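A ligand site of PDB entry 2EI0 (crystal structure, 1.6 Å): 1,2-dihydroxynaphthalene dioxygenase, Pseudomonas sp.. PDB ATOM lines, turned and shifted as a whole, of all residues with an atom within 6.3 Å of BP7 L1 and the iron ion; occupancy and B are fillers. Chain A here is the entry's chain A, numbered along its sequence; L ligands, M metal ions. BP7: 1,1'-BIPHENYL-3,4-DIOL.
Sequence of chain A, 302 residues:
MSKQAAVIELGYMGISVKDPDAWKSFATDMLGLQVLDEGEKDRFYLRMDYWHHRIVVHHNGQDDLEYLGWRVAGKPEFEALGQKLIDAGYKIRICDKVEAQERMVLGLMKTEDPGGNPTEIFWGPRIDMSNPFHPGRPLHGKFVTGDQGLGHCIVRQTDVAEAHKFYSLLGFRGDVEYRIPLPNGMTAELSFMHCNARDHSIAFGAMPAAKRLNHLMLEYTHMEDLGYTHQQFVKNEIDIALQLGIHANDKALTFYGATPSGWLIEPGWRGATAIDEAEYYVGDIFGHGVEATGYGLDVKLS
The side-chain hydroxyl of Tyr 256 is in hydrogen-bond range of the side-chain carboxylate of Glu 266.
OD1 of Asn 214 is in hydrogen-bond range of ND1 of His 215, 2.8 Å away.
A ring nitrogen (ND1) of His 152 lies close to a ring nitrogen (NE2) of His 200 (3.5 Å).
The backbone carbonyl oxygen of His 152 is in hydrogen-bond range of the backbone NH of Met 217 (2.8 Å).
OH of Tyr 256 sits close to NE2 of His 247, 3.3 Å away.
ND1 of His 200 lies within hydrogen-bond range of OD2 of Asp 199, 2.8 Å away.
OH of Tyr 178 lies within hydrogen-bond range of N of Asn 249 (3.0 Å).
OH of Tyr 178 sits at hydrogen-bond distance from N of Ala 248 (2.9 Å).
OE1 of Glu 266 is bound to the iron ion, at 2.0 Å.
An oxygen (OA3) of BP7 L1 is bound to the iron ion, at 2.1 Å.
NE2 of His 215 is bound to the iron ion (2.2 Å).
A ring nitrogen (NE2) of His 152 binds the iron ion (2.2 Å).
An oxygen (OA4) of BP7 L1 is bound to the iron ion (2.3 Å).
The iron ion has five donor atoms within binding distance.
Merely in contact with BP7 L1: Tyr 178 (3.3 Å), Ile 180 (3.996 Å), Leu 190 (3.3 Å), Phe 192 (3.5 Å), His 247 (3.1 Å), Asn 249 (3.3 Å) and Asp 284 (3.4 Å).
Hydrophobic or aromatic side chains within 4 Å of BP7 L1: His 152, Tyr 178, Ile 180, Leu 190, Phe 192, His 200, His 215, His 247 and Tyr 256.
Along chain A the residues within 4 Å of BP7 L1 span positions 152 to 284.
OA3 of BP7 L1 lies close to OH of Tyr 256 (2.4 Å).
NE2 of His 200 lies close to OA4 of BP7 L1 (2.6 Å).
Tyr 256 touches the iron ion (OH to FE, 3.5 Å).
Of the 22 residues printed, 4 come within 4 Å of the iron ion.
The nearest printed residue that does not touch the iron ion is Ile 154 (4.1 Å).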
ATOM      1  N   HIS A 152     -18.536 -23.978 -15.739  1.00  0.00           N
ATOM      2  CA  HIS A 152     -18.275 -25.421 -15.700  1.00  0.00           C
ATOM      3  C   HIS A 152     -19.248 -26.210 -16.553  1.00  0.00           C
ATOM      4  O   HIS A 152     -20.350 -25.741 -16.834  1.00  0.00           O
ATOM      5  CB  HIS A 152     -18.193 -25.987 -14.266  1.00  0.00           C
ATOM      6  CG  HIS A 152     -19.501 -26.066 -13.522  1.00  0.00           C
ATOM      7  ND1 HIS A 152     -19.742 -25.318 -12.389  1.00  0.00           N
ATOM      8  CD2 HIS A 152     -20.582 -26.872 -13.676  1.00  0.00           C
ATOM      9  CE1 HIS A 152     -20.932 -25.625 -11.903  1.00  0.00           C
ATOM     10  NE2 HIS A 152     -21.458 -26.578 -12.655  1.00  0.00           N
ATOM     11  N   ILE A 154     -20.884 -30.347 -17.087  1.00  0.00           N
ATOM     12  CA  ILE A 154     -20.969 -31.772 -16.776  1.00  0.00           C
ATOM     13  C   ILE A 154     -21.131 -32.454 -18.125  1.00  0.00           C
ATOM     14  O   ILE A 154     -22.015 -32.084 -18.893  1.00  0.00           O
ATOM     15  CB  ILE A 154     -22.174 -32.088 -15.854  1.00  0.00           C
ATOM     16  CG1 ILE A 154     -21.853 -31.784 -14.389  1.00  0.00           C
ATOM     17  CG2 ILE A 154     -22.569 -33.573 -15.964  1.00  0.00           C
ATOM     18  CD1 ILE A 154     -21.213 -30.411 -14.094  1.00  0.00           C
ATOM     19  N   TYR A 178     -20.079 -36.502  -4.309  1.00  0.00           N
ATOM     20  CA  TYR A 178     -21.411 -36.855  -3.829  1.00  0.00           C
ATOM     21  C   TYR A 178     -21.655 -38.330  -3.953  1.00  0.00           C
ATOM     22  O   TYR A 178     -21.292 -38.927  -4.971  1.00  0.00           O
ATOM     23  CB  TYR A 178     -22.502 -36.137  -4.611  1.00  0.00           C
ATOM     24  CG  TYR A 178     -22.613 -34.654  -4.318  1.00  0.00           C
ATOM     25  CD1 TYR A 178     -21.790 -33.750  -4.970  1.00  0.00           C
ATOM     26  CD2 TYR A 178     -23.535 -34.160  -3.394  1.00  0.00           C
ATOM     27  CE1 TYR A 178     -21.867 -32.385  -4.738  1.00  0.00           C
ATOM     28  CE2 TYR A 178     -23.616 -32.766  -3.146  1.00  0.00           C
ATOM     29  CZ  TYR A 178     -22.783 -31.906  -3.830  1.00  0.00           C
ATOM     30  OH  TYR A 178     -22.845 -30.528  -3.630  1.00  0.00           O
ATOM     31  N   ILE A 180     -25.040 -40.366  -3.745  1.00  0.00           N
ATOM     32  CA  ILE A 180     -26.480 -40.119  -3.683  1.00  0.00           C
ATOM     33  C   ILE A 180     -27.263 -41.438  -3.671  1.00  0.00           C
ATOM     34  O   ILE A 180     -27.138 -42.230  -4.612  1.00  0.00           O
ATOM     35  CB  ILE A 180     -26.949 -39.214  -4.860  1.00  0.00           C
ATOM     36  CG1 ILE A 180     -26.181 -37.873  -4.886  1.00  0.00           C
ATOM     37  CG2 ILE A 180     -28.472 -39.011  -4.804  1.00  0.00           C
ATOM     38  CD1 ILE A 180     -26.262 -37.048  -3.592  1.00  0.00           C
ATOM     39  N   LEU A 190     -20.769 -39.047  -7.950  1.00  0.00           N
ATOM     40  CA  LEU A 190     -20.527 -37.939  -8.879  1.00  0.00           C
ATOM     41  C   LEU A 190     -19.177 -37.326  -8.581  1.00  0.00           C
ATOM     42  O   LEU A 190     -18.909 -36.990  -7.426  1.00  0.00           O
ATOM     43  CB  LEU A 190     -21.616 -36.864  -8.751  1.00  0.00           C
ATOM     44  CG  LEU A 190     -23.062 -37.384  -8.724  1.00  0.00           C
ATOM     45  CD1 LEU A 190     -24.020 -36.218  -8.511  1.00  0.00           C
ATOM     46  CD2 LEU A 190     -23.424 -38.134  -9.981  1.00  0.00           C
ATOM     47  N   PHE A 192     -16.064 -34.427  -9.344  1.00  0.00           N
ATOM     48  CA  PHE A 192     -15.966 -33.003  -9.686  1.00  0.00           C
ATOM     49  C   PHE A 192     -14.508 -32.603  -9.664  1.00  0.00           C
ATOM     50  O   PHE A 192     -13.818 -32.876  -8.674  1.00  0.00           O
ATOM     51  CB  PHE A 192     -16.720 -32.129  -8.672  1.00  0.00           C
ATOM     52  CG  PHE A 192     -18.206 -32.383  -8.625  1.00  0.00           C
ATOM     53  CD1 PHE A 192     -18.715 -33.492  -7.929  1.00  0.00           C
ATOM     54  CD2 PHE A 192     -19.102 -31.489  -9.208  1.00  0.00           C
ATOM     55  CE1 PHE A 192     -20.090 -33.725  -7.871  1.00  0.00           C
ATOM     56  CE2 PHE A 192     -20.477 -31.730  -9.161  1.00  0.00           C
ATOM     57  CZ  PHE A 192     -20.962 -32.841  -8.480  1.00  0.00           C
ATOM     58  N   ASP A 199     -14.708 -23.736  -8.160  1.00  0.00           N
ATOM     59  CA  ASP A 199     -14.818 -24.971  -7.378  1.00  0.00           C
ATOM     60  C   ASP A 199     -14.740 -26.219  -8.263  1.00  0.00           C
ATOM     61  O   ASP A 199     -14.082 -27.193  -7.922  1.00  0.00           O
ATOM     62  CB  ASP A 199     -16.081 -25.016  -6.555  1.00  0.00           C
ATOM     63  CG  ASP A 199     -16.223 -26.328  -5.825  1.00  0.00           C
ATOM     64  OD1 ASP A 199     -15.603 -26.459  -4.741  1.00  0.00           O
ATOM     65  OD2 ASP A 199     -16.871 -27.238  -6.379  1.00  0.00           O
ATOM     66  N   HIS A 200     -15.435 -26.197  -9.397  1.00  0.00           N
ATOM     67  CA  HIS A 200     -15.207 -27.211 -10.409  1.00  0.00           C
ATOM     68  C   HIS A 200     -15.363 -26.610 -11.806  1.00  0.00           C
ATOM     69  O   HIS A 200     -16.115 -25.639 -11.980  1.00  0.00           O
ATOM     70  CB  HIS A 200     -16.095 -28.455 -10.245  1.00  0.00           C
ATOM     71  CG  HIS A 200     -17.555 -28.153 -10.025  1.00  0.00           C
ATOM     72  ND1 HIS A 200     -18.034 -27.621  -8.850  1.00  0.00           N
ATOM     73  CD2 HIS A 200     -18.642 -28.364 -10.817  1.00  0.00           C
ATOM     74  CE1 HIS A 200     -19.348 -27.494  -8.930  1.00  0.00           C
ATOM     75  NE2 HIS A 200     -19.738 -27.935 -10.103  1.00  0.00           N
ATOM     76  N   ASN A 214     -24.576 -32.381 -20.273  1.00  0.00           N
ATOM     77  CA  ASN A 214     -25.704 -32.341 -19.345  1.00  0.00           C
ATOM     78  C   ASN A 214     -26.092 -30.908 -19.029  1.00  0.00           C
ATOM     79  O   ASN A 214     -27.258 -30.523 -19.151  1.00  0.00           O
ATOM     80  CB  ASN A 214     -25.402 -33.068 -18.044  1.00  0.00           C
ATOM     81  CG  ASN A 214     -26.526 -32.933 -17.033  1.00  0.00           C
ATOM     82  OD1 ASN A 214     -26.448 -32.128 -16.092  1.00  0.00           O
ATOM     83  ND2 ASN A 214     -27.601 -33.684 -17.237  1.00  0.00           N
ATOM     84  N   HIS A 215     -25.111 -30.124 -18.597  1.00  0.00           N
ATOM     85  CA  HIS A 215     -25.354 -28.710 -18.328  1.00  0.00           C
ATOM     86  C   HIS A 215     -24.090 -27.894 -18.363  1.00  0.00           C
ATOM     87  O   HIS A 215     -22.987 -28.423 -18.203  1.00  0.00           O
ATOM     88  CB  HIS A 215     -26.120 -28.473 -16.998  1.00  0.00           C
ATOM     89  CG  HIS A 215     -25.306 -28.620 -15.753  1.00  0.00           C
ATOM     90  ND1 HIS A 215     -25.171 -29.833 -15.092  1.00  0.00           N
ATOM     91  CD2 HIS A 215     -24.638 -27.713 -14.998  1.00  0.00           C
ATOM     92  CE1 HIS A 215     -24.419 -29.654 -14.015  1.00  0.00           C
ATOM     93  NE2 HIS A 215     -24.095 -28.378 -13.935  1.00  0.00           N
ATOM     94  N   LEU A 216     -24.313 -26.600 -18.584  1.00  0.00           N
ATOM     95  CA  LEU A 216     -23.288 -25.572 -18.508  1.00  0.00           C
ATOM     96  C   LEU A 216     -23.710 -24.613 -17.396  1.00  0.00           C
ATOM     97  O   LEU A 216     -24.854 -24.148 -17.376  1.00  0.00           O
ATOM     98  CB  LEU A 216     -23.204 -24.817 -19.842  1.00  0.00           C
ATOM     99  CG  LEU A 216     -22.528 -23.447 -19.844  1.00  0.00           C
ATOM    100  CD1 LEU A 216     -21.024 -23.612 -19.542  1.00  0.00           C
ATOM    101  CD2 LEU A 216     -22.740 -22.778 -21.192  1.00  0.00           C
ATOM    102  N   MET A 217     -22.786 -24.323 -16.486  1.00  0.00           N
ATOM    103  CA  MET A 217     -23.018 -23.344 -15.437  1.00  0.00           C
ATOM    104  C   MET A 217     -22.319 -22.028 -15.787  1.00  0.00           C
ATOM    105  O   MET A 217     -21.133 -22.022 -16.121  1.00  0.00           O
ATOM    106  CB  MET A 217     -22.501 -23.880 -14.104  1.00  0.00           C
ATOM    107  CG  MET A 217     -22.857 -23.051 -12.871  1.00  0.00           C
ATOM    108  SD  MET A 217     -21.715 -21.699 -12.554  1.00  0.00           S
ATOM    109  CE  MET A 217     -22.625 -20.940 -11.203  1.00  0.00           C
ATOM    110  N   HIS A 247     -25.441 -25.724  -3.561  1.00  0.00           N
ATOM    111  CA  HIS A 247     -24.631 -26.925  -3.619  1.00  0.00           C
ATOM    112  C   HIS A 247     -23.756 -27.057  -2.401  1.00  0.00           C
ATOM    113  O   HIS A 247     -23.144 -26.075  -1.965  1.00  0.00           O
ATOM    114  CB  HIS A 247     -23.680 -26.846  -4.812  1.00  0.00           C
ATOM    115  CG  HIS A 247     -24.361 -26.908  -6.135  1.00  0.00           C
ATOM    116  ND1 HIS A 247     -25.218 -27.926  -6.473  1.00  0.00           N
ATOM    117  CD2 HIS A 247     -24.257 -26.113  -7.219  1.00  0.00           C
ATOM    118  CE1 HIS A 247     -25.637 -27.750  -7.710  1.00  0.00           C
ATOM    119  NE2 HIS A 247     -25.080 -26.646  -8.188  1.00  0.00           N
ATOM    120  N   ALA A 248     -23.634 -28.286  -1.887  1.00  0.00           N
ATOM    121  CA  ALA A 248     -22.734 -28.535  -0.746  1.00  0.00           C
ATOM    122  C   ALA A 248     -21.266 -28.323  -1.115  1.00  0.00           C
ATOM    123  O   ALA A 248     -20.492 -27.833  -0.295  1.00  0.00           O
ATOM    124  CB  ALA A 248     -22.957 -29.937  -0.169  1.00  0.00           C
ATOM    125  N   ASN A 249     -20.893 -28.650  -2.349  1.00  0.00           N
ATOM    126  CA  ASN A 249     -19.493 -28.456  -2.757  1.00  0.00           C
ATOM    127  C   ASN A 249     -19.082 -26.996  -3.038  1.00  0.00           C
ATOM    128  O   ASN A 249     -18.224 -26.466  -2.342  1.00  0.00           O
ATOM    129  CB  ASN A 249     -19.021 -29.432  -3.866  1.00  0.00           C
ATOM    130  CG  ASN A 249     -19.832 -29.343  -5.150  1.00  0.00           C
ATOM    131  OD1 ASN A 249     -20.696 -28.477  -5.326  1.00  0.00           O
ATOM    132  ND2 ASN A 249     -19.519 -30.254  -6.084  1.00  0.00           N
ATOM    133  N   ASP A 250     -19.711 -26.338  -4.024  1.00  0.00           N
ATOM    134  CA  ASP A 250     -19.270 -24.988  -4.362  1.00  0.00           C
ATOM    135  C   ASP A 250     -19.992 -23.854  -3.648  1.00  0.00           C
ATOM    136  O   ASP A 250     -19.608 -22.687  -3.799  1.00  0.00           O
ATOM    137  CB  ASP A 250     -19.221 -24.745  -5.862  1.00  0.00           C
ATOM    138  CG  ASP A 250     -20.590 -24.607  -6.513  1.00  0.00           C
ATOM    139  OD1 ASP A 250     -21.650 -24.663  -5.833  1.00  0.00           O
ATOM    140  OD2 ASP A 250     -20.593 -24.439  -7.744  1.00  0.00           O
ATOM    141  N   THR A 254     -27.890 -21.527  -7.225  1.00  0.00           N
ATOM    142  CA  THR A 254     -28.106 -21.788  -8.649  1.00  0.00           C
ATOM    143  C   THR A 254     -29.473 -22.427  -8.890  1.00  0.00           C
ATOM    144  O   THR A 254     -30.086 -22.984  -7.960  1.00  0.00           O
ATOM    145  CB  THR A 254     -27.048 -22.766  -9.243  1.00  0.00           C
ATOM    146  OG1 THR A 254     -27.440 -24.120  -8.960  1.00  0.00           O
ATOM    147  CG2 THR A 254     -25.612 -22.522  -8.711  1.00  0.00           C
ATOM    148  N   TYR A 256     -31.523 -24.682 -12.470  1.00  0.00           N
ATOM    149  CA  TYR A 256     -31.240 -25.274 -13.782  1.00  0.00           C
ATOM    150  C   TYR A 256     -32.445 -25.104 -14.692  1.00  0.00           C
ATOM    151  O   TYR A 256     -33.554 -25.483 -14.320  1.00  0.00           O
ATOM    152  CB  TYR A 256     -30.940 -26.775 -13.674  1.00  0.00           C
ATOM    153  CG  TYR A 256     -29.730 -27.167 -12.843  1.00  0.00           C
ATOM    154  CD1 TYR A 256     -29.683 -26.944 -11.453  1.00  0.00           C
ATOM    155  CD2 TYR A 256     -28.646 -27.799 -13.458  1.00  0.00           C
ATOM    156  CE1 TYR A 256     -28.573 -27.324 -10.713  1.00  0.00           C
ATOM    157  CE2 TYR A 256     -27.530 -28.186 -12.721  1.00  0.00           C
ATOM    158  CZ  TYR A 256     -27.512 -27.962 -11.349  1.00  0.00           C
ATOM    159  OH  TYR A 256     -26.408 -28.363 -10.628  1.00  0.00           O
ATOM    160  N   GLU A 266     -27.253 -23.681 -16.098  1.00  0.00           N
ATOM    161  CA  GLU A 266     -27.309 -23.486 -14.667  1.00  0.00           C
ATOM    162  C   GLU A 266     -26.807 -22.081 -14.341  1.00  0.00           C
ATOM    163  O   GLU A 266     -25.616 -21.884 -14.104  1.00  0.00           O
ATOM    164  CB  GLU A 266     -26.454 -24.550 -13.954  1.00  0.00           C
ATOM    165  CG  GLU A 266     -26.492 -24.453 -12.430  1.00  0.00           C
ATOM    166  CD  GLU A 266     -25.481 -25.365 -11.720  1.00  0.00           C
ATOM    167  OE1 GLU A 266     -24.595 -25.956 -12.385  1.00  0.00           O
ATOM    168  OE2 GLU A 266     -25.571 -25.448 -10.474  1.00  0.00           O
ATOM    169  N   GLY A 283     -25.959 -34.937  -0.009  1.00  0.00           N
ATOM    170  CA  GLY A 283     -27.049 -34.076  -0.455  1.00  0.00           C
ATOM    171  C   GLY A 283     -26.662 -32.607  -0.435  1.00  0.00           C
ATOM    172  O   GLY A 283     -25.594 -32.245   0.099  1.00  0.00           O
ATOM    173  N   ASP A 284     -27.516 -31.773  -1.022  1.00  0.00           N
ATOM    174  CA  ASP A 284     -27.204 -30.343  -1.086  1.00  0.00           C
ATOM    175  C   ASP A 284     -27.638 -29.613   0.208  1.00  0.00           C
ATOM    176  O   ASP A 284     -28.231 -30.222   1.111  1.00  0.00           O
ATOM    177  CB  ASP A 284     -27.757 -29.719  -2.382  1.00  0.00           C
ATOM    178  CG  ASP A 284     -26.648 -29.556  -3.459  1.00  0.00           C
ATOM    179  OD1 ASP A 284     -25.470 -29.925  -3.191  1.00  0.00           O
ATOM    180  OD2 ASP A 284     -26.945 -29.038  -4.566  1.00  0.00           O
ATOM    181  N   HIS A 288     -32.832 -27.129  -4.915  1.00  0.00           N
ATOM    182  CA  HIS A 288     -32.504 -27.975  -6.071  1.00  0.00           C
ATOM    183  C   HIS A 288     -33.473 -29.143  -6.185  1.00  0.00           C
ATOM    184  O   HIS A 288     -33.088 -30.251  -6.575  1.00  0.00           O
ATOM    185  CB  HIS A 288     -31.057 -28.454  -6.024  1.00  0.00           C
ATOM    186  CG  HIS A 288     -30.056 -27.385  -6.371  1.00  0.00           C
ATOM    187  ND1 HIS A 288     -28.792 -27.349  -5.828  1.00  0.00           N
ATOM    188  CD2 HIS A 288     -30.141 -26.329  -7.210  1.00  0.00           C
ATOM    189  CE1 HIS A 288     -28.146 -26.301  -6.304  1.00  0.00           C
ATOM    190  NE2 HIS A 288     -28.927 -25.670  -7.156  1.00  0.00           N
HETATM  191  CA1 BP7 L   1     -24.160 -30.891  -7.988  1.00  0.00           C
HETATM  192  CA2 BP7 L   1     -24.497 -30.580  -9.299  1.00  0.00           C
HETATM  193  CA3 BP7 L   1     -23.868 -29.557  -9.968  1.00  0.00           C
HETATM  194  OA3 BP7 L   1     -24.250 -29.292 -11.250  1.00  0.00           O
HETATM  195  CA4 BP7 L   1     -22.880 -28.797  -9.338  1.00  0.00           C
HETATM  196  OA4 BP7 L   1     -22.290 -27.771 -10.041  1.00  0.00           O
HETATM  197  CA5 BP7 L   1     -22.520 -29.087  -8.006  1.00  0.00           C
HETATM  198  CA6 BP7 L   1     -23.168 -30.137  -7.338  1.00  0.00           C
HETATM  199  CB1 BP7 L   1     -24.938 -31.982  -7.345  1.00  0.00           C
HETATM  200  CB2 BP7 L   1     -25.433 -33.057  -8.072  1.00  0.00           C
HETATM  201  CB3 BP7 L   1     -26.213 -34.035  -7.448  1.00  0.00           C
HETATM  202  CB4 BP7 L   1     -26.522 -33.943  -6.094  1.00  0.00           C
HETATM  203  CB5 BP7 L   1     -26.049 -32.852  -5.353  1.00  0.00           C
HETATM  204  CB6 BP7 L   1     -25.285 -31.866  -5.990  1.00  0.00           C
HETATM  205  CA1 BP7 L   2     -25.494 -35.535 -13.768  1.00  0.00           C
HETATM  206  CA2 BP7 L   2     -25.311 -36.063 -15.062  1.00  0.00           C
HETATM  207  CA3 BP7 L   2     -26.397 -36.556 -15.789  1.00  0.00           C
HETATM  208  OA3 BP7 L   2     -26.221 -37.069 -17.043  1.00  0.00           O
HETATM  209  CA4 BP7 L   2     -27.671 -36.515 -15.219  1.00  0.00           C
HETATM  210  OA4 BP7 L   2     -28.745 -36.987 -15.918  1.00  0.00           O
HETATM  211  CA5 BP7 L   2     -27.871 -35.993 -13.938  1.00  0.00           C
HETATM  212  CA6 BP7 L   2     -26.779 -35.507 -13.215  1.00  0.00           C
HETATM  213  CB1 BP7 L   2     -24.327 -35.018 -12.997  1.00  0.00           C
HETATM  214  CB2 BP7 L   2     -23.112 -35.723 -13.045  1.00  0.00           C
HETATM  215  CB3 BP7 L   2     -22.004 -35.260 -12.332  1.00  0.00           C
HETATM  216  CB4 BP7 L   2     -22.096 -34.099 -11.559  1.00  0.00           C
HETATM  217  CB5 BP7 L   2     -23.294 -33.388 -11.499  1.00  0.00           C
HETATM  218  CB6 BP7 L   2     -24.407 -33.851 -12.220  1.00  0.00           C
HETATM  219 FE    FE M   1     -23.358 -27.519 -12.072  1.00  0.00          FE
